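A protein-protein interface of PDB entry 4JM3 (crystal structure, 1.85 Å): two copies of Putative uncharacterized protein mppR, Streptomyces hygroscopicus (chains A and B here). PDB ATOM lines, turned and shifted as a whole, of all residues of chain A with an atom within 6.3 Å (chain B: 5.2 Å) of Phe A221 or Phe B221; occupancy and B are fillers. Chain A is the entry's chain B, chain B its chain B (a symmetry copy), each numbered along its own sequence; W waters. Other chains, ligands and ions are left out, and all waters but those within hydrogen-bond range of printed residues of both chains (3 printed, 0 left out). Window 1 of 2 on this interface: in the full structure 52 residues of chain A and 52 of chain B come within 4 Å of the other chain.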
ATOM      1  N   TYR A  38       6.474   8.120  19.509  1.00  0.00           N
ATOM      2  CA  TYR A  38       5.885   8.076  18.172  1.00  0.00           C
ATOM      3  C   TYR A  38       6.918   8.459  17.116  1.00  0.00           C
ATOM      4  O   TYR A  38       6.917   7.929  16.007  1.00  0.00           O
ATOM      5  CB  TYR A  38       4.656   9.004  18.084  1.00  0.00           C
ATOM      6  CG  TYR A  38       4.052   9.015  16.703  1.00  0.00           C
ATOM      7  CD1 TYR A  38       3.454   7.878  16.186  1.00  0.00           C
ATOM      8  CD2 TYR A  38       4.123  10.152  15.901  1.00  0.00           C
ATOM      9  CE1 TYR A  38       2.929   7.869  14.915  1.00  0.00           C
ATOM     10  CE2 TYR A  38       3.605  10.160  14.630  1.00  0.00           C
ATOM     11  CZ  TYR A  38       3.002   9.023  14.143  1.00  0.00           C
ATOM     12  OH  TYR A  38       2.484   9.034  12.877  1.00  0.00           O
ATOM     13  N   SER A  39       7.793   9.400  17.467  1.00  0.00           N
ATOM     14  CA  SER A  39       8.890   9.834  16.611  1.00  0.00           C
ATOM     15  C   SER A  39      10.062  10.268  17.482  1.00  0.00           C
ATOM     16  O   SER A  39       9.940  10.351  18.702  1.00  0.00           O
ATOM     17  CB  SER A  39       8.470  11.030  15.727  1.00  0.00           C
ATOM     18  OG  SER A  39       8.408  12.246  16.446  1.00  0.00           O
ATOM     19  N   MET A 147       7.729  17.904   8.910  1.00  0.00           N
ATOM     20  CA  MET A 147       8.080  16.517   9.195  1.00  0.00           C
ATOM     21  C   MET A 147       6.861  15.606   9.079  1.00  0.00           C
ATOM     22  O   MET A 147       6.950  14.502   8.534  1.00  0.00           O
ATOM     23  CB  MET A 147       8.708  16.374  10.582  1.00  0.00           C
ATOM     24  CG  MET A 147       9.339  15.014  10.831  1.00  0.00           C
ATOM     25  SD  MET A 147      10.730  14.686   9.750  1.00  0.00           S
ATOM     26  CE  MET A 147      11.946  15.813  10.443  1.00  0.00           C
ATOM     27  N   TRP A 150       6.252  14.642   5.599  1.00  0.00           N
ATOM     28  CA  TRP A 150       7.066  13.533   5.118  1.00  0.00           C
ATOM     29  C   TRP A 150       6.534  12.199   5.633  1.00  0.00           C
ATOM     30  O   TRP A 150       6.586  11.184   4.932  1.00  0.00           O
ATOM     31  CB  TRP A 150       8.542  13.724   5.475  1.00  0.00           C
ATOM     32  CG  TRP A 150       9.229  14.729   4.599  1.00  0.00           C
ATOM     33  CD1 TRP A 150       8.765  15.964   4.251  1.00  0.00           C
ATOM     34  CD2 TRP A 150      10.503  14.581   3.961  1.00  0.00           C
ATOM     35  NE1 TRP A 150       9.674  16.594   3.428  1.00  0.00           N
ATOM     36  CE2 TRP A 150      10.749  15.765   3.234  1.00  0.00           C
ATOM     37  CE3 TRP A 150      11.455  13.563   3.931  1.00  0.00           C
ATOM     38  CZ2 TRP A 150      11.915  15.963   2.496  1.00  0.00           C
ATOM     39  CZ3 TRP A 150      12.619  13.758   3.184  1.00  0.00           C
ATOM     40  CH2 TRP A 150      12.838  14.946   2.483  1.00  0.00           C
ATOM     41  N   VAL A 151       5.980  12.188   6.840  1.00  0.00           N
ATOM     42  CA  VAL A 151       5.464  10.947   7.398  1.00  0.00           C
ATOM     43  C   VAL A 151       4.370  10.369   6.505  1.00  0.00           C
ATOM     44  O   VAL A 151       4.275   9.140   6.324  1.00  0.00           O
ATOM     45  CB  VAL A 151       4.913  11.131   8.813  1.00  0.00           C
ATOM     46  CG1 VAL A 151       4.033   9.947   9.195  1.00  0.00           C
ATOM     47  CG2 VAL A 151       6.051  11.322   9.818  1.00  0.00           C
ATOM     48  N   GLN A 152       3.562  11.248   5.925  1.00  0.00           N
ATOM     49  CA  GLN A 152       2.437  10.806   5.090  1.00  0.00           C
ATOM     50  C   GLN A 152       2.781  10.808   3.582  1.00  0.00           C
ATOM     51  O   GLN A 152       1.929  10.532   2.736  1.00  0.00           O
ATOM     52  CB  GLN A 152       1.189  11.653   5.411  1.00  0.00           C
ATOM     53  CG  GLN A 152       1.254  13.083   4.943  1.00  0.00           C
ATOM     54  CD  GLN A 152       0.342  14.023   5.753  1.00  0.00           C
ATOM     55  OE1 GLN A 152       0.640  14.392   6.898  1.00  0.00           O
ATOM     56  NE2 GLN A 152      -0.747  14.426   5.150  1.00  0.00           N
ATOM     57  N   LEU A 219       5.362   7.173  -0.121  1.00  0.00           N
ATOM     58  CA  LEU A 219       6.113   7.034   1.126  1.00  0.00           C
ATOM     59  C   LEU A 219       7.506   6.583   0.809  1.00  0.00           C
ATOM     60  O   LEU A 219       7.709   5.455   0.335  1.00  0.00           O
ATOM     61  CB  LEU A 219       5.492   5.999   2.061  1.00  0.00           C
ATOM     62  CG  LEU A 219       4.136   6.270   2.682  1.00  0.00           C
ATOM     63  CD1 LEU A 219       3.796   5.121   3.629  1.00  0.00           C
ATOM     64  CD2 LEU A 219       4.116   7.629   3.395  1.00  0.00           C
ATOM     65  N   VAL A 220       8.467   7.464   1.053  1.00  0.00           N
ATOM     66  CA  VAL A 220       9.858   7.098   0.904  1.00  0.00           C
ATOM     67  C   VAL A 220      10.753   8.018   1.752  1.00  0.00           C
ATOM     68  O   VAL A 220      10.504   9.222   1.906  1.00  0.00           O
ATOM     69  CB  VAL A 220      10.267   7.100  -0.587  1.00  0.00           C
ATOM     70  CG1 VAL A 220      10.283   8.513  -1.132  1.00  0.00           C
ATOM     71  CG2 VAL A 220      11.606   6.421  -0.772  1.00  0.00           C
ATOM     72  N   PHE A 221      11.793   7.426   2.322  1.00  0.00           N
ATOM     73  CA  PHE A 221      12.698   8.161   3.202  1.00  0.00           C
ATOM     74  C   PHE A 221      14.105   7.682   2.881  1.00  0.00           C
ATOM     75  O   PHE A 221      14.309   6.507   2.621  1.00  0.00           O
ATOM     76  CB  PHE A 221      12.337   7.873   4.658  1.00  0.00           C
ATOM     77  CG  PHE A 221      12.914   8.852   5.629  1.00  0.00           C
ATOM     78  CD1 PHE A 221      12.535  10.186   5.597  1.00  0.00           C
ATOM     79  CD2 PHE A 221      13.814   8.443   6.590  1.00  0.00           C
ATOM     80  CE1 PHE A 221      13.075  11.093   6.493  1.00  0.00           C
ATOM     81  CE2 PHE A 221      14.335   9.365   7.502  1.00  0.00           C
ATOM     82  CZ  PHE A 221      13.971  10.672   7.439  1.00  0.00           C
ATOM     83  N   PRO A 222      15.085   8.588   2.877  1.00  0.00           N
ATOM     84  CA  PRO A 222      16.407   8.113   2.467  1.00  0.00           C
ATOM     85  C   PRO A 222      16.949   6.999   3.341  1.00  0.00           C
ATOM     86  O   PRO A 222      16.697   6.955   4.556  1.00  0.00           O
ATOM     87  CB  PRO A 222      17.278   9.364   2.606  1.00  0.00           C
ATOM     88  CG  PRO A 222      16.355  10.469   2.439  1.00  0.00           C
ATOM     89  CD  PRO A 222      15.061  10.044   3.063  1.00  0.00           C
ATOM     90  N   GLU A 223      17.701   6.109   2.700  1.00  0.00           N
ATOM     91  CA  GLU A 223      18.401   5.031   3.375  1.00  0.00           C
ATOM     92  C   GLU A 223      19.769   5.538   3.797  1.00  0.00           C
ATOM     93  O   GLU A 223      20.526   6.072   2.991  1.00  0.00           O
ATOM     94  CB  GLU A 223      18.558   3.828   2.434  1.00  0.00           C
ATOM     95  CG  GLU A 223      17.673   2.646   2.778  1.00  0.00           C
ATOM     96  CD  GLU A 223      17.685   1.572   1.702  1.00  0.00           C
ATOM     97  OE1 GLU A 223      16.936   0.584   1.849  1.00  0.00           O
ATOM     98  OE2 GLU A 223      18.437   1.716   0.710  1.00  0.00           O
ATOM     99  N   PRO A 231      15.902   2.152  -0.651  1.00  0.00           N
ATOM    100  CA  PRO A 231      14.559   2.636  -0.335  1.00  0.00           C
ATOM    101  C   PRO A 231      13.490   1.802  -1.035  1.00  0.00           C
ATOM    102  O   PRO A 231      13.678   1.426  -2.193  1.00  0.00           O
ATOM    103  CB  PRO A 231      14.579   4.052  -0.912  1.00  0.00           C
ATOM    104  CG  PRO A 231      15.535   3.950  -2.112  1.00  0.00           C
ATOM    105  CD  PRO A 231      16.354   2.678  -1.947  1.00  0.00           C
ATOM    106  N   ARG A 232      12.394   1.506  -0.342  1.00  0.00           N
ATOM    107  CA  ARG A 232      11.264   0.819  -0.964  1.00  0.00           C
ATOM    108  C   ARG A 232      10.008   1.694  -0.875  1.00  0.00           C
ATOM    109  O   ARG A 232       9.273   1.655   0.110  1.00  0.00           O
ATOM    110  CB  ARG A 232      11.020  -0.560  -0.340  1.00  0.00           C
ATOM    111  CG  ARG A 232      11.800  -0.843   0.940  1.00  0.00           C
ATOM    112  CD  ARG A 232      12.194  -2.321   1.060  1.00  0.00           C
ATOM    113  NE  ARG A 232      13.349  -2.656   0.221  1.00  0.00           N
ATOM    114  CZ  ARG A 232      14.163  -3.691   0.422  1.00  0.00           C
ATOM    115  NH1 ARG A 232      13.971  -4.521   1.442  1.00  0.00           N
ATOM    116  NH2 ARG A 232      15.185  -3.897  -0.401  1.00  0.00           N
ATOM    117  N   MET B 147      15.980  17.795   8.624  1.00  0.00           N
ATOM    118  CA  MET B 147      15.581  16.567   7.949  1.00  0.00           C
ATOM    119  C   MET B 147      16.766  15.618   7.787  1.00  0.00           C
ATOM    120  O   MET B 147      16.635  14.407   7.985  1.00  0.00           O
ATOM    121  CB  MET B 147      14.956  16.858   6.583  1.00  0.00           C
ATOM    122  CG  MET B 147      14.278  15.653   5.952  1.00  0.00           C
ATOM    123  SD  MET B 147      12.871  15.073   6.897  1.00  0.00           S
ATOM    124  CE  MET B 147      11.699  16.396   6.570  1.00  0.00           C
ATOM    125  N   TRP B 150      17.322  13.658  10.830  1.00  0.00           N
ATOM    126  CA  TRP B 150      16.466  12.487  10.970  1.00  0.00           C
ATOM    127  C   TRP B 150      16.953  11.344  10.085  1.00  0.00           C
ATOM    128  O   TRP B 150      16.861  10.170  10.460  1.00  0.00           O
ATOM    129  CB  TRP B 150      15.000  12.827  10.692  1.00  0.00           C
ATOM    130  CG  TRP B 150      14.345  13.555  11.828  1.00  0.00           C
ATOM    131  CD1 TRP B 150      14.850  14.617  12.519  1.00  0.00           C
ATOM    132  CD2 TRP B 150      13.063  13.273  12.401  1.00  0.00           C
ATOM    133  NE1 TRP B 150      13.960  15.012  13.495  1.00  0.00           N
ATOM    134  CE2 TRP B 150      12.855  14.202  13.444  1.00  0.00           C
ATOM    135  CE3 TRP B 150      12.075  12.325  12.137  1.00  0.00           C
ATOM    136  CZ2 TRP B 150      11.693  14.217  14.213  1.00  0.00           C
ATOM    137  CZ3 TRP B 150      10.915  12.335  12.915  1.00  0.00           C
ATOM    138  CH2 TRP B 150      10.734  13.274  13.934  1.00  0.00           C
ATOM    139  N   VAL B 151      17.513  11.666   8.924  1.00  0.00           N
ATOM    140  CA  VAL B 151      17.987  10.623   8.025  1.00  0.00           C
ATOM    141  C   VAL B 151      19.054   9.772   8.705  1.00  0.00           C
ATOM    142  O   VAL B 151      19.105   8.541   8.519  1.00  0.00           O
ATOM    143  CB  VAL B 151      18.551  11.194   6.724  1.00  0.00           C
ATOM    144  CG1 VAL B 151      19.391  10.143   6.007  1.00  0.00           C
ATOM    145  CG2 VAL B 151      17.426  11.711   5.824  1.00  0.00           C
ATOM    146  N   LEU B 219      17.914   4.816  14.113  1.00  0.00           N
ATOM    147  CA  LEU B 219      17.165   5.075  12.884  1.00  0.00           C
ATOM    148  C   LEU B 219      15.755   4.601  13.063  1.00  0.00           C
ATOM    149  O   LEU B 219      15.509   3.392  13.187  1.00  0.00           O
ATOM    150  CB  LEU B 219      17.753   4.337  11.684  1.00  0.00           C
ATOM    151  CG  LEU B 219      19.121   4.730  11.162  1.00  0.00           C
ATOM    152  CD1 LEU B 219      19.425   3.896   9.920  1.00  0.00           C
ATOM    153  CD2 LEU B 219      19.194   6.235  10.878  1.00  0.00           C
ATOM    154  N   VAL B 220      14.828   5.548  13.092  1.00  0.00           N
ATOM    155  CA  VAL B 220      13.423   5.205  13.135  1.00  0.00           C
ATOM    156  C   VAL B 220      12.566   6.365  12.598  1.00  0.00           C
ATOM    157  O   VAL B 220      12.859   7.551  12.801  1.00  0.00           O
ATOM    158  CB  VAL B 220      13.007   4.786  14.563  1.00  0.00           C
ATOM    159  CG1 VAL B 220      13.038   5.978  15.498  1.00  0.00           C
ATOM    160  CG2 VAL B 220      11.643   4.131  14.549  1.00  0.00           C
ATOM    161  N   PHE B 221      11.509   6.002  11.885  1.00  0.00           N
ATOM    162  CA  PHE B 221      10.636   6.994  11.263  1.00  0.00           C
ATOM    163  C   PHE B 221       9.210   6.493  11.438  1.00  0.00           C
ATOM    164  O   PHE B 221       8.963   5.302  11.344  1.00  0.00           O
ATOM    165  CB  PHE B 221      10.994   7.132   9.784  1.00  0.00           C
ATOM    166  CG  PHE B 221      10.458   8.371   9.145  1.00  0.00           C
ATOM    167  CD1 PHE B 221      10.884   9.624   9.563  1.00  0.00           C
ATOM    168  CD2 PHE B 221       9.548   8.294   8.111  1.00  0.00           C
ATOM    169  CE1 PHE B 221      10.382  10.771   8.974  1.00  0.00           C
ATOM    170  CE2 PHE B 221       9.066   9.459   7.511  1.00  0.00           C
ATOM    171  CZ  PHE B 221       9.475  10.678   7.951  1.00  0.00           C
ATOM    172  N   PRO B 222       8.264   7.393  11.711  1.00  0.00           N
ATOM    173  CA  PRO B 222       6.923   6.867  11.972  1.00  0.00           C
ATOM    174  C   PRO B 222       6.347   6.076  10.814  1.00  0.00           C
ATOM    175  O   PRO B 222       6.603   6.381   9.638  1.00  0.00           O
ATOM    176  CB  PRO B 222       6.099   8.134  12.209  1.00  0.00           C
ATOM    177  CG  PRO B 222       7.059   9.108  12.688  1.00  0.00           C
ATOM    178  CD  PRO B 222       8.341   8.838  11.959  1.00  0.00           C
ATOM    179  N   GLU B 223       5.559   5.066  11.171  1.00  0.00           N
ATOM    180  CA  GLU B 223       4.825   4.257  10.213  1.00  0.00           C
ATOM    181  C   GLU B 223       3.479   4.914   9.965  1.00  0.00           C
ATOM    182  O   GLU B 223       2.736   5.216  10.897  1.00  0.00           O
ATOM    183  CB  GLU B 223       4.620   2.839  10.764  1.00  0.00           C
ATOM    184  CG  GLU B 223       5.464   1.777  10.084  1.00  0.00           C
ATOM    185  CD  GLU B 223       5.408   0.438  10.800  1.00  0.00           C
ATOM    186  OE1 GLU B 223       6.122  -0.490  10.365  1.00  0.00           O
ATOM    187  OE2 GLU B 223       4.657   0.312  11.794  1.00  0.00           O
ATOM    188  N   PRO B 231       7.198   0.240  13.209  1.00  0.00           N
ATOM    189  CA  PRO B 231       8.560   0.748  13.041  1.00  0.00           C
ATOM    190  C   PRO B 231       9.594  -0.292  13.461  1.00  0.00           C
ATOM    191  O   PRO B 231       9.386  -0.983  14.460  1.00  0.00           O
ATOM    192  CB  PRO B 231       8.587   1.933  14.007  1.00  0.00           C
ATOM    193  CG  PRO B 231       7.621   1.519  15.130  1.00  0.00           C
ATOM    194  CD  PRO B 231       6.758   0.380  14.605  1.00  0.00           C
HETATM  195  O   HOH W   1      17.267   6.934   7.419  1.00  0.00           O
HETATM  196  O   HOH W   2       6.048   7.217   6.896  1.00  0.00           O
HETATM  197  O   HOH W   3       1.348   6.881  12.070  1.00  0.00           O
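Tyr A38 touches Pro B222.
Ser A39 touches Trp B150 (OG to CH2, 3.6 Å).
CB of Ser A39 touches CG of Pro B222 (3.9 Å).
Trp A150 touches Met B147.
CE2 of Phe B221 touches O of Trp A150, at 3.97 Å.
Val A151 touches Phe B221.
Val A151 touches Pro B222.
O of Trp B150 touches CE2 of Phe A221, at 3.97 Å.
Phe A221 touches Val B151 (CE2 to CA, 3.9 Å).
CE1 of Phe A221 touches CE1 of Phe B221, at 3.7 Å.
Hydrophobic or aromatic side chains of chain B within 4 Å of the printed part of chain A: Met B147, Trp B150, Val B151, Phe B221 and Pro B222.
Among the printed residues, 13 pairs touch across the chains.
Water W3 lies within hydrogen-bond range of O of Glu B223 (2.5 Å) and OH of Tyr A38 (2.6 Å).
Water W1 lies within hydrogen-bond range of the backbone carbonyl oxygen (O) of Val B151 and the backbone carbonyl oxygen (O) of Pro A222.
Water W2 bridges the backbone carbonyl oxygen (O) of Val A151 (2.7 Å) and the backbone carbonyl oxygen (O) of Pro B222 (2.9 Å).
SD of Met A147 sits close to SD of Met B147, at 3.6 Å.
Met B147 touches its own counterpart, Met A147.
Met A147 touches Trp B150, and with the chains exchanged Trp A150 touches Met B147.
Trp A150 touches Phe B221, and with the chains exchanged Phe A221 touches Trp B150.
Val A151 touches Pro B222, and with the chains exchanged Pro A222 touches Val B151.
9 positions are printed for both chains.
Of the 13 pairs that touch across the chains among the printed residues, 10 have their exchanged pair printed and touching as well.
Of the printed residues of chain B, Val A151 touches Phe B221 and Pro B222.
Of the printed residues of chain B, Phe A221 touches Trp B150 (3.97 Å), Val B151 (3.9 Å) and Phe B221 (3.7 Å).
Printed residues of chain B within 4 Å of Pro A222: Val B151.
Of the printed residues of chain A, Phe B221 touches Trp A150 (3.97 Å), Val A151 (3.9 Å) and Phe A221 (3.7 Å).
The nearest printed residue of chain B that does not touch Phe A221 is Met B147 (4.01 Å).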
